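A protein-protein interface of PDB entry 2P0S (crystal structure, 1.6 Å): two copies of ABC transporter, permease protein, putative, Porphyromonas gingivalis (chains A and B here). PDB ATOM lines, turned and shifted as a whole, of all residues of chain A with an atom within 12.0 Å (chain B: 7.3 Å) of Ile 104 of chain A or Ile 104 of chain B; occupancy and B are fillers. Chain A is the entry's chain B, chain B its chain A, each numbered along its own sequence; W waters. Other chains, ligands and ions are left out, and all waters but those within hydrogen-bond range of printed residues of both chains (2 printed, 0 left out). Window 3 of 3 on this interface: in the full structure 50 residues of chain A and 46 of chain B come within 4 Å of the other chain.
The backbone carbonyl oxygen of Ile 110 of chain A sits at hydrogen-bond distance from the side-chain hydroxyl of Ser 114 of chain A (2.8 Å).
The side-chain amide oxygen of Gln 109 of chain A sits close to the side-chain carboxylate of Asp 113 of chain A (3.0 Å).
Among the printed residues, merely in contact across the chains: Ile 99 of chain A with Ile 110 of chain B, Tyr 102 of chain A with Ile 110 of chain B, Ile 104 of chain A with Ile 104 of chain B, Ile 110 of chain A with Tyr 102 of chain B, Leu 111 of chain A with Ile 99 of chain B, Asp 113 of chain A with Tyr 102 of chain B, Ser 114 of chain A with Ile 99 of chain B and Ser 114 of chain A with Tyr 102 of chain B.
Ile 104 of chain A touches just one residue of chain B: Ile 104 (3.7 Å).
Of chain A, only Ile 104 comes within 4 Å of Ile 104 of chain B.
No residue of chain A comes within 4 Å of Asn 103 of chain B.
No residue of chain A comes within 4 Å of Pro 105 of chain B.
No residue of chain A comes within 4 Å of Asp 106 of chain B.
No residue of chain A comes within 4 Å of Ile 107 of chain B.
Of the printed residues of chain B, Ile 110 of chain A touches Tyr 102.
Of the printed residues of chain B, Tyr 102 of chain A touches Ile 110 (3.6 Å).
The nearest residue of chain A that does not touch Ile 104 of chain B is Ile 110 of chain A (4.1 Å).
Printed residues of chain B that touch a printed residue of chain A: Ile 99, Tyr 102, Ile 104 and Ile 110.
Hydrophobic or aromatic side chains of chain B that line the printed part of chain A: Ile 99, Tyr 102, Ile 104 and Ile 110.
Hydrophobic or aromatic side chains of chain A within 4 Å of the printed part of chain B: Ile 99, Tyr 102, Ile 104, Ile 110 and Leu 111.
Among the printed residues, no Asp or Glu carboxylate lies within 4 Å of a Lys or Arg side-chain nitrogen of the other chain.
Ile 99 of chain A touches Ile 110 of chain B, but with the chains exchanged Ile 110 of chain A does not touch Ile 99 of chain B (4.2 Å).
Tyr 102 of chain A touches Ile 110 of chain B, and with the chains exchanged Ile 110 of chain A touches Tyr 102 of chain B.
Ile 104 of chain B touches its own counterpart, Ile 104 of chain A.
12 positions are printed for both chains.
Of the 8 pairs that touch across the chains among the printed residues, 3 have their exchanged pair printed and touching as well.
Water W2 bridges the side-chain carboxylate (OD2) of Asp 113 of chain A (2.6 Å) and the side-chain hydroxyl (OH) of Tyr 102 of chain B (2.7 Å).
Water W1 bridges OH of Tyr 102 of chain B (2.7 Å) and OG of Ser 114 of chain A (3.2 Å).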
ATOM      1  N   SER A  95      26.000  18.251  29.069  1.00  0.00           N
ATOM      2  CA  SER A  95      24.537  18.269  28.876  1.00  0.00           C
ATOM      3  C   SER A  95      24.244  17.983  27.389  1.00  0.00           C
ATOM      4  O   SER A  95      23.351  17.149  27.073  1.00  0.00           O
ATOM      5  CB  SER A  95      24.011  19.611  29.246  1.00  0.00           C
ATOM      6  OG  SER A  95      24.278  19.888  30.673  1.00  0.00           O
ATOM      7  N   ASP A  96      24.982  18.618  26.488  1.00  0.00           N
ATOM      8  CA  ASP A  96      24.733  18.359  25.011  1.00  0.00           C
ATOM      9  C   ASP A  96      24.950  16.901  24.717  1.00  0.00           C
ATOM     10  O   ASP A  96      24.215  16.300  23.894  1.00  0.00           O
ATOM     11  CB  ASP A  96      25.679  19.228  24.181  1.00  0.00           C
ATOM     12  CG  ASP A  96      25.279  20.733  24.164  1.00  0.00           C
ATOM     13  OD1 ASP A  96      24.189  21.087  24.683  1.00  0.00           O
ATOM     14  OD2 ASP A  96      26.072  21.587  23.585  1.00  0.00           O
ATOM     15  N   LYS A  97      26.014  16.340  25.296  1.00  0.00           N
ATOM     16  CA  LYS A  97      26.418  14.941  24.976  1.00  0.00           C
ATOM     17  C   LYS A  97      25.302  13.995  25.505  1.00  0.00           C
ATOM     18  O   LYS A  97      24.903  13.027  24.843  1.00  0.00           O
ATOM     19  CB  LYS A  97      27.756  14.601  25.589  1.00  0.00           C
ATOM     20  CG  LYS A  97      28.270  13.225  25.062  1.00  0.00           C
ATOM     21  CD  LYS A  97      29.756  13.073  25.204  1.00  0.00           C
ATOM     22  CE  LYS A  97      30.242  11.683  24.792  1.00  0.00           C
ATOM     23  NZ  LYS A  97      31.243  11.922  23.742  1.00  0.00           N
ATOM     24  N   LYS A  98      24.822  14.255  26.740  1.00  0.00           N
ATOM     25  CA  LYS A  98      23.799  13.372  27.279  1.00  0.00           C
ATOM     26  C   LYS A  98      22.476  13.463  26.430  1.00  0.00           C
ATOM     27  O   LYS A  98      21.922  12.400  26.114  1.00  0.00           O
ATOM     28  CB  LYS A  98      23.484  13.785  28.685  1.00  0.00           C
ATOM     29  CG  LYS A  98      22.527  12.780  29.399  1.00  0.00           C
ATOM     30  CD  LYS A  98      22.516  13.049  30.949  1.00  0.00           C
ATOM     31  CE  LYS A  98      21.306  12.186  31.568  1.00  0.00           C
ATOM     32  NZ  LYS A  98      21.280  12.473  33.067  1.00  0.00           N
ATOM     33  N   ILE A  99      21.984  14.640  26.007  1.00  0.00           N
ATOM     34  CA  ILE A  99      20.733  14.680  25.313  1.00  0.00           C
ATOM     35  C   ILE A  99      21.051  14.000  23.947  1.00  0.00           C
ATOM     36  O   ILE A  99      20.108  13.351  23.344  1.00  0.00           O
ATOM     37  CB  ILE A  99      20.159  16.121  25.119  1.00  0.00           C
ATOM     38  CG1 ILE A  99      18.791  16.035  24.380  1.00  0.00           C
ATOM     39  CG2 ILE A  99      21.162  17.017  24.396  1.00  0.00           C
ATOM     40  CD1 ILE A  99      17.799  15.184  25.089  1.00  0.00           C
ATOM     41  N   ALA A 100      22.281  14.193  23.455  1.00  0.00           N
ATOM     42  CA  ALA A 100      22.598  13.605  22.115  1.00  0.00           C
ATOM     43  C   ALA A 100      22.612  12.059  22.145  1.00  0.00           C
ATOM     44  O   ALA A 100      22.698  11.418  21.063  1.00  0.00           O
ATOM     45  CB  ALA A 100      23.930  14.145  21.649  1.00  0.00           C
ATOM     46  N   SER A 101      22.646  11.459  23.331  1.00  0.00           N
ATOM     47  CA  SER A 101      22.642   9.993  23.439  1.00  0.00           C
ATOM     48  C   SER A 101      21.184   9.431  23.308  1.00  0.00           C
ATOM     49  O   SER A 101      21.020   8.232  23.336  1.00  0.00           O
ATOM     50  CB  SER A 101      23.269   9.588  24.807  1.00  0.00           C
ATOM     51  OG  SER A 101      22.456   9.969  25.915  1.00  0.00           O
ATOM     52  N   TYR A 102      20.156  10.308  23.394  1.00  0.00           N
ATOM     53  CA  TYR A 102      18.766   9.870  23.624  1.00  0.00           C
ATOM     54  C   TYR A 102      18.235   9.059  22.478  1.00  0.00           C
ATOM     55  O   TYR A 102      18.673   9.337  21.372  1.00  0.00           O
ATOM     56  CB  TYR A 102      17.857  11.067  24.009  1.00  0.00           C
ATOM     57  CG  TYR A 102      16.786  10.604  24.971  1.00  0.00           C
ATOM     58  CD1 TYR A 102      17.056  10.523  26.399  1.00  0.00           C
ATOM     59  CD2 TYR A 102      15.480  10.348  24.497  1.00  0.00           C
ATOM     60  CE1 TYR A 102      16.043  10.153  27.261  1.00  0.00           C
ATOM     61  CE2 TYR A 102      14.455   9.925  25.371  1.00  0.00           C
ATOM     62  CZ  TYR A 102      14.741   9.862  26.766  1.00  0.00           C
ATOM     63  OH  TYR A 102      13.751   9.471  27.607  1.00  0.00           O
ATOM     64  N   ASN A 103      17.351   8.046  22.730  1.00  0.00           N
ATOM     65  CA  ASN A 103      16.968   7.102  21.612  1.00  0.00           C
ATOM     66  C   ASN A 103      15.689   7.657  20.946  1.00  0.00           C
ATOM     67  O   ASN A 103      14.554   7.174  21.073  1.00  0.00           O
ATOM     68  CB  ASN A 103      16.768   5.772  22.265  1.00  0.00           C
ATOM     69  CG  ASN A 103      16.349   4.732  21.205  1.00  0.00           C
ATOM     70  OD1 ASN A 103      16.600   5.040  20.056  1.00  0.00           O
ATOM     71  ND2 ASN A 103      15.860   3.552  21.607  1.00  0.00           N
ATOM     72  N   ILE A 104      15.918   8.752  20.210  1.00  0.00           N
ATOM     73  CA  ILE A 104      14.954   9.373  19.225  1.00  0.00           C
ATOM     74  C   ILE A 104      15.673   9.419  17.913  1.00  0.00           C
ATOM     75  O   ILE A 104      16.772   9.901  17.853  1.00  0.00           O
ATOM     76  CB  ILE A 104      14.667  10.829  19.673  1.00  0.00           C
ATOM     77  CG1 ILE A 104      13.885  10.826  21.000  1.00  0.00           C
ATOM     78  CG2 ILE A 104      13.902  11.545  18.485  1.00  0.00           C
ATOM     79  CD1 ILE A 104      14.157  12.041  21.769  1.00  0.00           C
ATOM     80  N   PRO A 105      15.121   8.822  16.818  1.00  0.00           N
ATOM     81  CA  PRO A 105      16.019   8.477  15.694  1.00  0.00           C
ATOM     82  C   PRO A 105      16.743   9.687  15.055  1.00  0.00           C
ATOM     83  O   PRO A 105      17.912   9.554  14.529  1.00  0.00           O
ATOM     84  CB  PRO A 105      15.036   7.770  14.686  1.00  0.00           C
ATOM     85  CG  PRO A 105      13.660   8.269  15.096  1.00  0.00           C
ATOM     86  CD  PRO A 105      13.753   8.394  16.608  1.00  0.00           C
ATOM     87  N   ASP A 106      16.071  10.830  15.084  1.00  0.00           N
ATOM     88  CA  ASP A 106      16.698  12.005  14.417  1.00  0.00           C
ATOM     89  C   ASP A 106      17.151  13.029  15.494  1.00  0.00           C
ATOM     90  O   ASP A 106      17.205  14.250  15.187  1.00  0.00           O
ATOM     91  CB  ASP A 106      15.757  12.685  13.417  1.00  0.00           C
ATOM     92  CG  ASP A 106      14.335  12.930  13.963  1.00  0.00           C
ATOM     93  OD1 ASP A 106      14.013  12.528  15.101  1.00  0.00           O
ATOM     94  OD2 ASP A 106      13.461  13.503  13.201  1.00  0.00           O
ATOM     95  N   ILE A 107      17.483  12.557  16.706  1.00  0.00           N
ATOM     96  CA  ILE A 107      17.859  13.587  17.725  1.00  0.00           C
ATOM     97  C   ILE A 107      19.055  14.421  17.304  1.00  0.00           C
ATOM     98  O   ILE A 107      19.145  15.600  17.619  1.00  0.00           O
ATOM     99  CB  ILE A 107      18.076  12.942  19.115  1.00  0.00           C
ATOM    100  CG1 ILE A 107      18.165  13.992  20.262  1.00  0.00           C
ATOM    101  CG2 ILE A 107      19.308  11.969  19.151  1.00  0.00           C
ATOM    102  CD1 ILE A 107      16.977  14.800  20.347  1.00  0.00           C
ATOM    103  N   LYS A 108      20.016  13.835  16.595  1.00  0.00           N
ATOM    104  CA  LYS A 108      21.206  14.628  16.292  1.00  0.00           C
ATOM    105  C   LYS A 108      20.886  15.740  15.292  1.00  0.00           C
ATOM    106  O   LYS A 108      21.404  16.833  15.425  1.00  0.00           O
ATOM    107  CB  LYS A 108      22.383  13.770  15.881  1.00  0.00           C
ATOM    108  CG  LYS A 108      22.978  12.888  17.074  1.00  0.00           C
ATOM    109  CD  LYS A 108      24.430  12.370  16.933  1.00  0.00           C
ATOM    110  CE  LYS A 108      24.371  11.424  15.778  1.00  0.00           C
ATOM    111  NZ  LYS A 108      25.483  10.543  15.669  1.00  0.00           N
ATOM    112  N   GLN A 109      20.037  15.478  14.278  1.00  0.00           N
ATOM    113  CA  GLN A 109      19.551  16.519  13.389  1.00  0.00           C
ATOM    114  C   GLN A 109      18.828  17.606  14.206  1.00  0.00           C
ATOM    115  O   GLN A 109      19.043  18.826  14.041  1.00  0.00           O
ATOM    116  CB  GLN A 109      18.558  15.970  12.345  1.00  0.00           C
ATOM    117  CG  GLN A 109      18.054  17.190  11.602  1.00  0.00           C
ATOM    118  CD  GLN A 109      17.012  16.936  10.524  1.00  0.00           C
ATOM    119  OE1 GLN A 109      16.334  17.867  10.032  1.00  0.00           O
ATOM    120  NE2 GLN A 109      16.875  15.700  10.174  1.00  0.00           N
ATOM    121  N   ILE A 110      17.996  17.169  15.146  1.00  0.00           N
ATOM    122  CA  ILE A 110      17.123  18.105  15.891  1.00  0.00           C
ATOM    123  C   ILE A 110      18.037  18.987  16.722  1.00  0.00           C
ATOM    124  O   ILE A 110      17.839  20.214  16.767  1.00  0.00           O
ATOM    125  CB  ILE A 110      16.101  17.318  16.779  1.00  0.00           C
ATOM    126  CG1 ILE A 110      15.022  16.718  15.832  1.00  0.00           C
ATOM    127  CG2 ILE A 110      15.471  18.305  17.846  1.00  0.00           C
ATOM    128  CD1 ILE A 110      14.059  15.691  16.616  1.00  0.00           C
ATOM    129  N   LEU A 111      19.008  18.363  17.370  1.00  0.00           N
ATOM    130  CA  LEU A 111      19.918  19.153  18.216  1.00  0.00           C
ATOM    131  C   LEU A 111      20.721  20.141  17.383  1.00  0.00           C
ATOM    132  O   LEU A 111      20.941  21.279  17.786  1.00  0.00           O
ATOM    133  CB  LEU A 111      20.877  18.256  18.981  1.00  0.00           C
ATOM    134  CG  LEU A 111      20.124  17.366  20.003  1.00  0.00           C
ATOM    135  CD1 LEU A 111      21.075  16.335  20.689  1.00  0.00           C
ATOM    136  CD2 LEU A 111      19.337  18.252  20.962  1.00  0.00           C
ATOM    137  N   ALA A 112      21.241  19.705  16.230  1.00  0.00           N
ATOM    138  CA  ALA A 112      22.050  20.586  15.398  1.00  0.00           C
ATOM    139  C   ALA A 112      21.202  21.726  14.828  1.00  0.00           C
ATOM    140  O   ALA A 112      21.679  22.941  14.791  1.00  0.00           O
ATOM    141  CB  ALA A 112      22.693  19.709  14.245  1.00  0.00           C
ATOM    142  N   ASP A 113      20.001  21.371  14.339  1.00  0.00           N
ATOM    143  CA  ASP A 113      19.082  22.365  13.766  1.00  0.00           C
ATOM    144  C   ASP A 113      18.684  23.429  14.815  1.00  0.00           C
ATOM    145  O   ASP A 113      18.444  24.599  14.456  1.00  0.00           O
ATOM    146  CB  ASP A 113      17.861  21.715  13.311  1.00  0.00           C
ATOM    147  CG  ASP A 113      18.066  20.996  11.998  1.00  0.00           C
ATOM    148  OD1 ASP A 113      19.112  21.100  11.413  1.00  0.00           O
ATOM    149  OD2 ASP A 113      17.112  20.283  11.585  1.00  0.00           O
ATOM    150  N   SER A 114      18.621  23.028  16.076  1.00  0.00           N
ATOM    151  CA  SER A 114      18.115  23.876  17.164  1.00  0.00           C
ATOM    152  C   SER A 114      19.202  24.589  17.844  1.00  0.00           C
ATOM    153  O   SER A 114      18.942  25.445  18.731  1.00  0.00           O
ATOM    154  CB  SER A 114      17.439  22.983  18.223  1.00  0.00           C
ATOM    155  OG  SER A 114      16.313  22.349  17.702  1.00  0.00           O
ATOM    156  N   ILE B  99      14.234  22.861  20.602  1.00  0.00           N
ATOM    157  CA  ILE B  99      14.149  21.368  20.742  1.00  0.00           C
ATOM    158  C   ILE B  99      12.734  20.986  21.177  1.00  0.00           C
ATOM    159  O   ILE B  99      12.094  20.040  20.627  1.00  0.00           O
ATOM    160  CB  ILE B  99      15.171  20.788  21.759  1.00  0.00           C
ATOM    161  CG1 ILE B  99      16.627  21.002  21.236  1.00  0.00           C
ATOM    162  CG2 ILE B  99      14.943  19.236  21.941  1.00  0.00           C
ATOM    163  CD1 ILE B  99      17.710  20.901  22.393  1.00  0.00           C
ATOM    164  N   ALA B 100      12.199  21.673  22.194  1.00  0.00           N
ATOM    165  CA  ALA B 100      10.894  21.308  22.696  1.00  0.00           C
ATOM    166  C   ALA B 100       9.736  21.469  21.734  1.00  0.00           C
ATOM    167  O   ALA B 100       8.697  20.956  22.023  1.00  0.00           O
ATOM    168  CB  ALA B 100      10.639  22.149  24.016  1.00  0.00           C
ATOM    169  N   SER B 101       9.915  22.157  20.583  1.00  0.00           N
ATOM    170  CA  SER B 101       8.875  22.412  19.592  1.00  0.00           C
ATOM    171  C   SER B 101       8.702  21.163  18.645  1.00  0.00           C
ATOM    172  O   SER B 101       7.722  21.149  17.836  1.00  0.00           O
ATOM    173  CB  SER B 101       9.241  23.644  18.714  1.00  0.00           C
ATOM    174  OG  SER B 101      10.314  23.396  17.867  1.00  0.00           O
ATOM    175  N   TYR B 102       9.637  20.186  18.715  1.00  0.00           N
ATOM    176  CA  TYR B 102       9.512  18.934  17.850  1.00  0.00           C
ATOM    177  C   TYR B 102       8.502  18.004  18.546  1.00  0.00           C
ATOM    178  O   TYR B 102       8.096  18.203  19.702  1.00  0.00           O
ATOM    179  CB  TYR B 102      10.881  18.338  17.800  1.00  0.00           C
ATOM    180  CG  TYR B 102      11.748  19.195  16.860  1.00  0.00           C
ATOM    181  CD1 TYR B 102      11.886  18.781  15.500  1.00  0.00           C
ATOM    182  CD2 TYR B 102      12.491  20.321  17.334  1.00  0.00           C
ATOM    183  CE1 TYR B 102      12.613  19.523  14.663  1.00  0.00           C
ATOM    184  CE2 TYR B 102      13.280  21.062  16.511  1.00  0.00           C
ATOM    185  CZ  TYR B 102      13.317  20.674  15.167  1.00  0.00           C
ATOM    186  OH  TYR B 102      14.107  21.363  14.278  1.00  0.00           O
ATOM    187  N   ASN B 103       8.146  16.932  17.884  1.00  0.00           N
ATOM    188  CA  ASN B 103       7.063  16.101  18.404  1.00  0.00           C
ATOM    189  C   ASN B 103       7.663  14.963  19.218  1.00  0.00           C
ATOM    190  O   ASN B 103       7.884  13.816  18.698  1.00  0.00           O
ATOM    191  CB  ASN B 103       6.279  15.581  17.210  1.00  0.00           C
ATOM    192  CG  ASN B 103       5.614  16.694  16.416  1.00  0.00           C
ATOM    193  OD1 ASN B 103       5.250  17.741  16.956  1.00  0.00           O
ATOM    194  ND2 ASN B 103       5.369  16.434  15.063  1.00  0.00           N
ATOM    195  N   ILE B 104       8.014  15.220  20.473  1.00  0.00           N
ATOM    196  CA  ILE B 104       8.618  14.227  21.197  1.00  0.00           C
ATOM    197  C   ILE B 104       7.955  14.185  22.561  1.00  0.00           C
ATOM    198  O   ILE B 104       7.899  15.256  23.200  1.00  0.00           O
ATOM    199  CB  ILE B 104      10.158  14.605  21.515  1.00  0.00           C
ATOM    200  CG1 ILE B 104      10.969  14.741  20.169  1.00  0.00           C
ATOM    201  CG2 ILE B 104      10.799  13.501  22.364  1.00  0.00           C
ATOM    202  CD1 ILE B 104      12.204  15.520  20.290  1.00  0.00           C
ATOM    203  N   PRO B 105       7.442  13.041  22.958  1.00  0.00           N
ATOM    204  CA  PRO B 105       6.631  13.058  24.181  1.00  0.00           C
ATOM    205  C   PRO B 105       7.507  13.299  25.357  1.00  0.00           C
ATOM    206  O   PRO B 105       8.580  12.804  25.381  1.00  0.00           O
ATOM    207  CB  PRO B 105       6.027  11.665  24.230  1.00  0.00           C
ATOM    208  CG  PRO B 105       6.888  10.766  23.319  1.00  0.00           C
ATOM    209  CD  PRO B 105       7.349  11.729  22.260  1.00  0.00           C
ATOM    210  N   ASP B 106       6.983  14.082  26.279  1.00  0.00           N
ATOM    211  CA  ASP B 106       7.766  14.358  27.544  1.00  0.00           C
ATOM    212  C   ASP B 106       9.113  15.094  27.323  1.00  0.00           C
ATOM    213  O   ASP B 106      10.071  15.032  28.153  1.00  0.00           O
ATOM    214  CB  ASP B 106       7.991  13.151  28.368  1.00  0.00           C
ATOM    215  CG  ASP B 106       6.758  12.769  29.227  1.00  0.00           C
ATOM    216  OD1 ASP B 106       7.033  12.039  30.244  1.00  0.00           O
ATOM    217  OD2 ASP B 106       5.625  13.253  28.990  1.00  0.00           O
ATOM    218  N   ILE B 107       9.186  15.833  26.194  1.00  0.00           N
ATOM    219  CA  ILE B 107      10.460  16.474  25.864  1.00  0.00           C
ATOM    220  C   ILE B 107      10.894  17.460  26.984  1.00  0.00           C
ATOM    221  O   ILE B 107      12.092  17.562  27.281  1.00  0.00           O
ATOM    222  CB  ILE B 107      10.462  17.077  24.441  1.00  0.00           C
ATOM    223  CG1 ILE B 107      11.908  17.551  24.022  1.00  0.00           C
ATOM    224  CG2 ILE B 107       9.370  18.176  24.317  1.00  0.00           C
ATOM    225  CD1 ILE B 107      13.051  16.587  24.133  1.00  0.00           C
ATOM    226  N   LYS B 108       9.966  18.189  27.558  1.00  0.00           N
ATOM    227  CA  LYS B 108      10.470  19.095  28.656  1.00  0.00           C
ATOM    228  C   LYS B 108      11.127  18.349  29.752  1.00  0.00           C
ATOM    229  O   LYS B 108      12.178  18.801  30.239  1.00  0.00           O
ATOM    230  CB  LYS B 108       9.364  19.961  29.211  1.00  0.00           C
ATOM    231  CG  LYS B 108       8.976  20.979  28.128  1.00  0.00           C
ATOM    232  CD  LYS B 108       8.039  22.030  28.706  1.00  0.00           C
ATOM    233  CE  LYS B 108       6.817  22.254  27.778  1.00  0.00           C
ATOM    234  NZ  LYS B 108       5.801  23.338  28.313  1.00  0.00           N
ATOM    235  N   GLN B 109      10.546  17.199  30.151  1.00  0.00           N
ATOM    236  CA  GLN B 109      11.125  16.397  31.243  1.00  0.00           C
ATOM    237  C   GLN B 109      12.465  15.828  30.821  1.00  0.00           C
ATOM    238  O   GLN B 109      13.433  15.789  31.573  1.00  0.00           O
ATOM    239  CB  GLN B 109      10.155  15.266  31.700  1.00  0.00           C
ATOM    240  CG  GLN B 109       8.805  15.782  32.333  1.00  0.00           C
ATOM    241  CD  GLN B 109       7.923  16.808  31.535  1.00  0.00           C
ATOM    242  OE1 GLN B 109       7.378  17.814  32.178  1.00  0.00           O
ATOM    243  NE2 GLN B 109       7.722  16.580  30.169  1.00  0.00           N
ATOM    244  N   ILE B 110      12.516  15.291  29.581  1.00  0.00           N
ATOM    245  CA  ILE B 110      13.759  14.807  29.110  1.00  0.00           C
ATOM    246  C   ILE B 110      14.869  15.887  29.046  1.00  0.00           C
ATOM    247  O   ILE B 110      15.982  15.601  29.425  1.00  0.00           O
ATOM    248  CB  ILE B 110      13.590  14.179  27.691  1.00  0.00           C
ATOM    249  CG1 ILE B 110      12.716  12.954  27.828  1.00  0.00           C
ATOM    250  CG2 ILE B 110      14.940  13.860  27.089  1.00  0.00           C
ATOM    251  CD1 ILE B 110      12.158  12.554  26.391  1.00  0.00           C
HETATM  252  O   HOH W   1      15.010  23.773  15.106  1.00  0.00           O
HETATM  253  O   HOH W   2      14.481  20.480  11.756  1.00  0.00           O
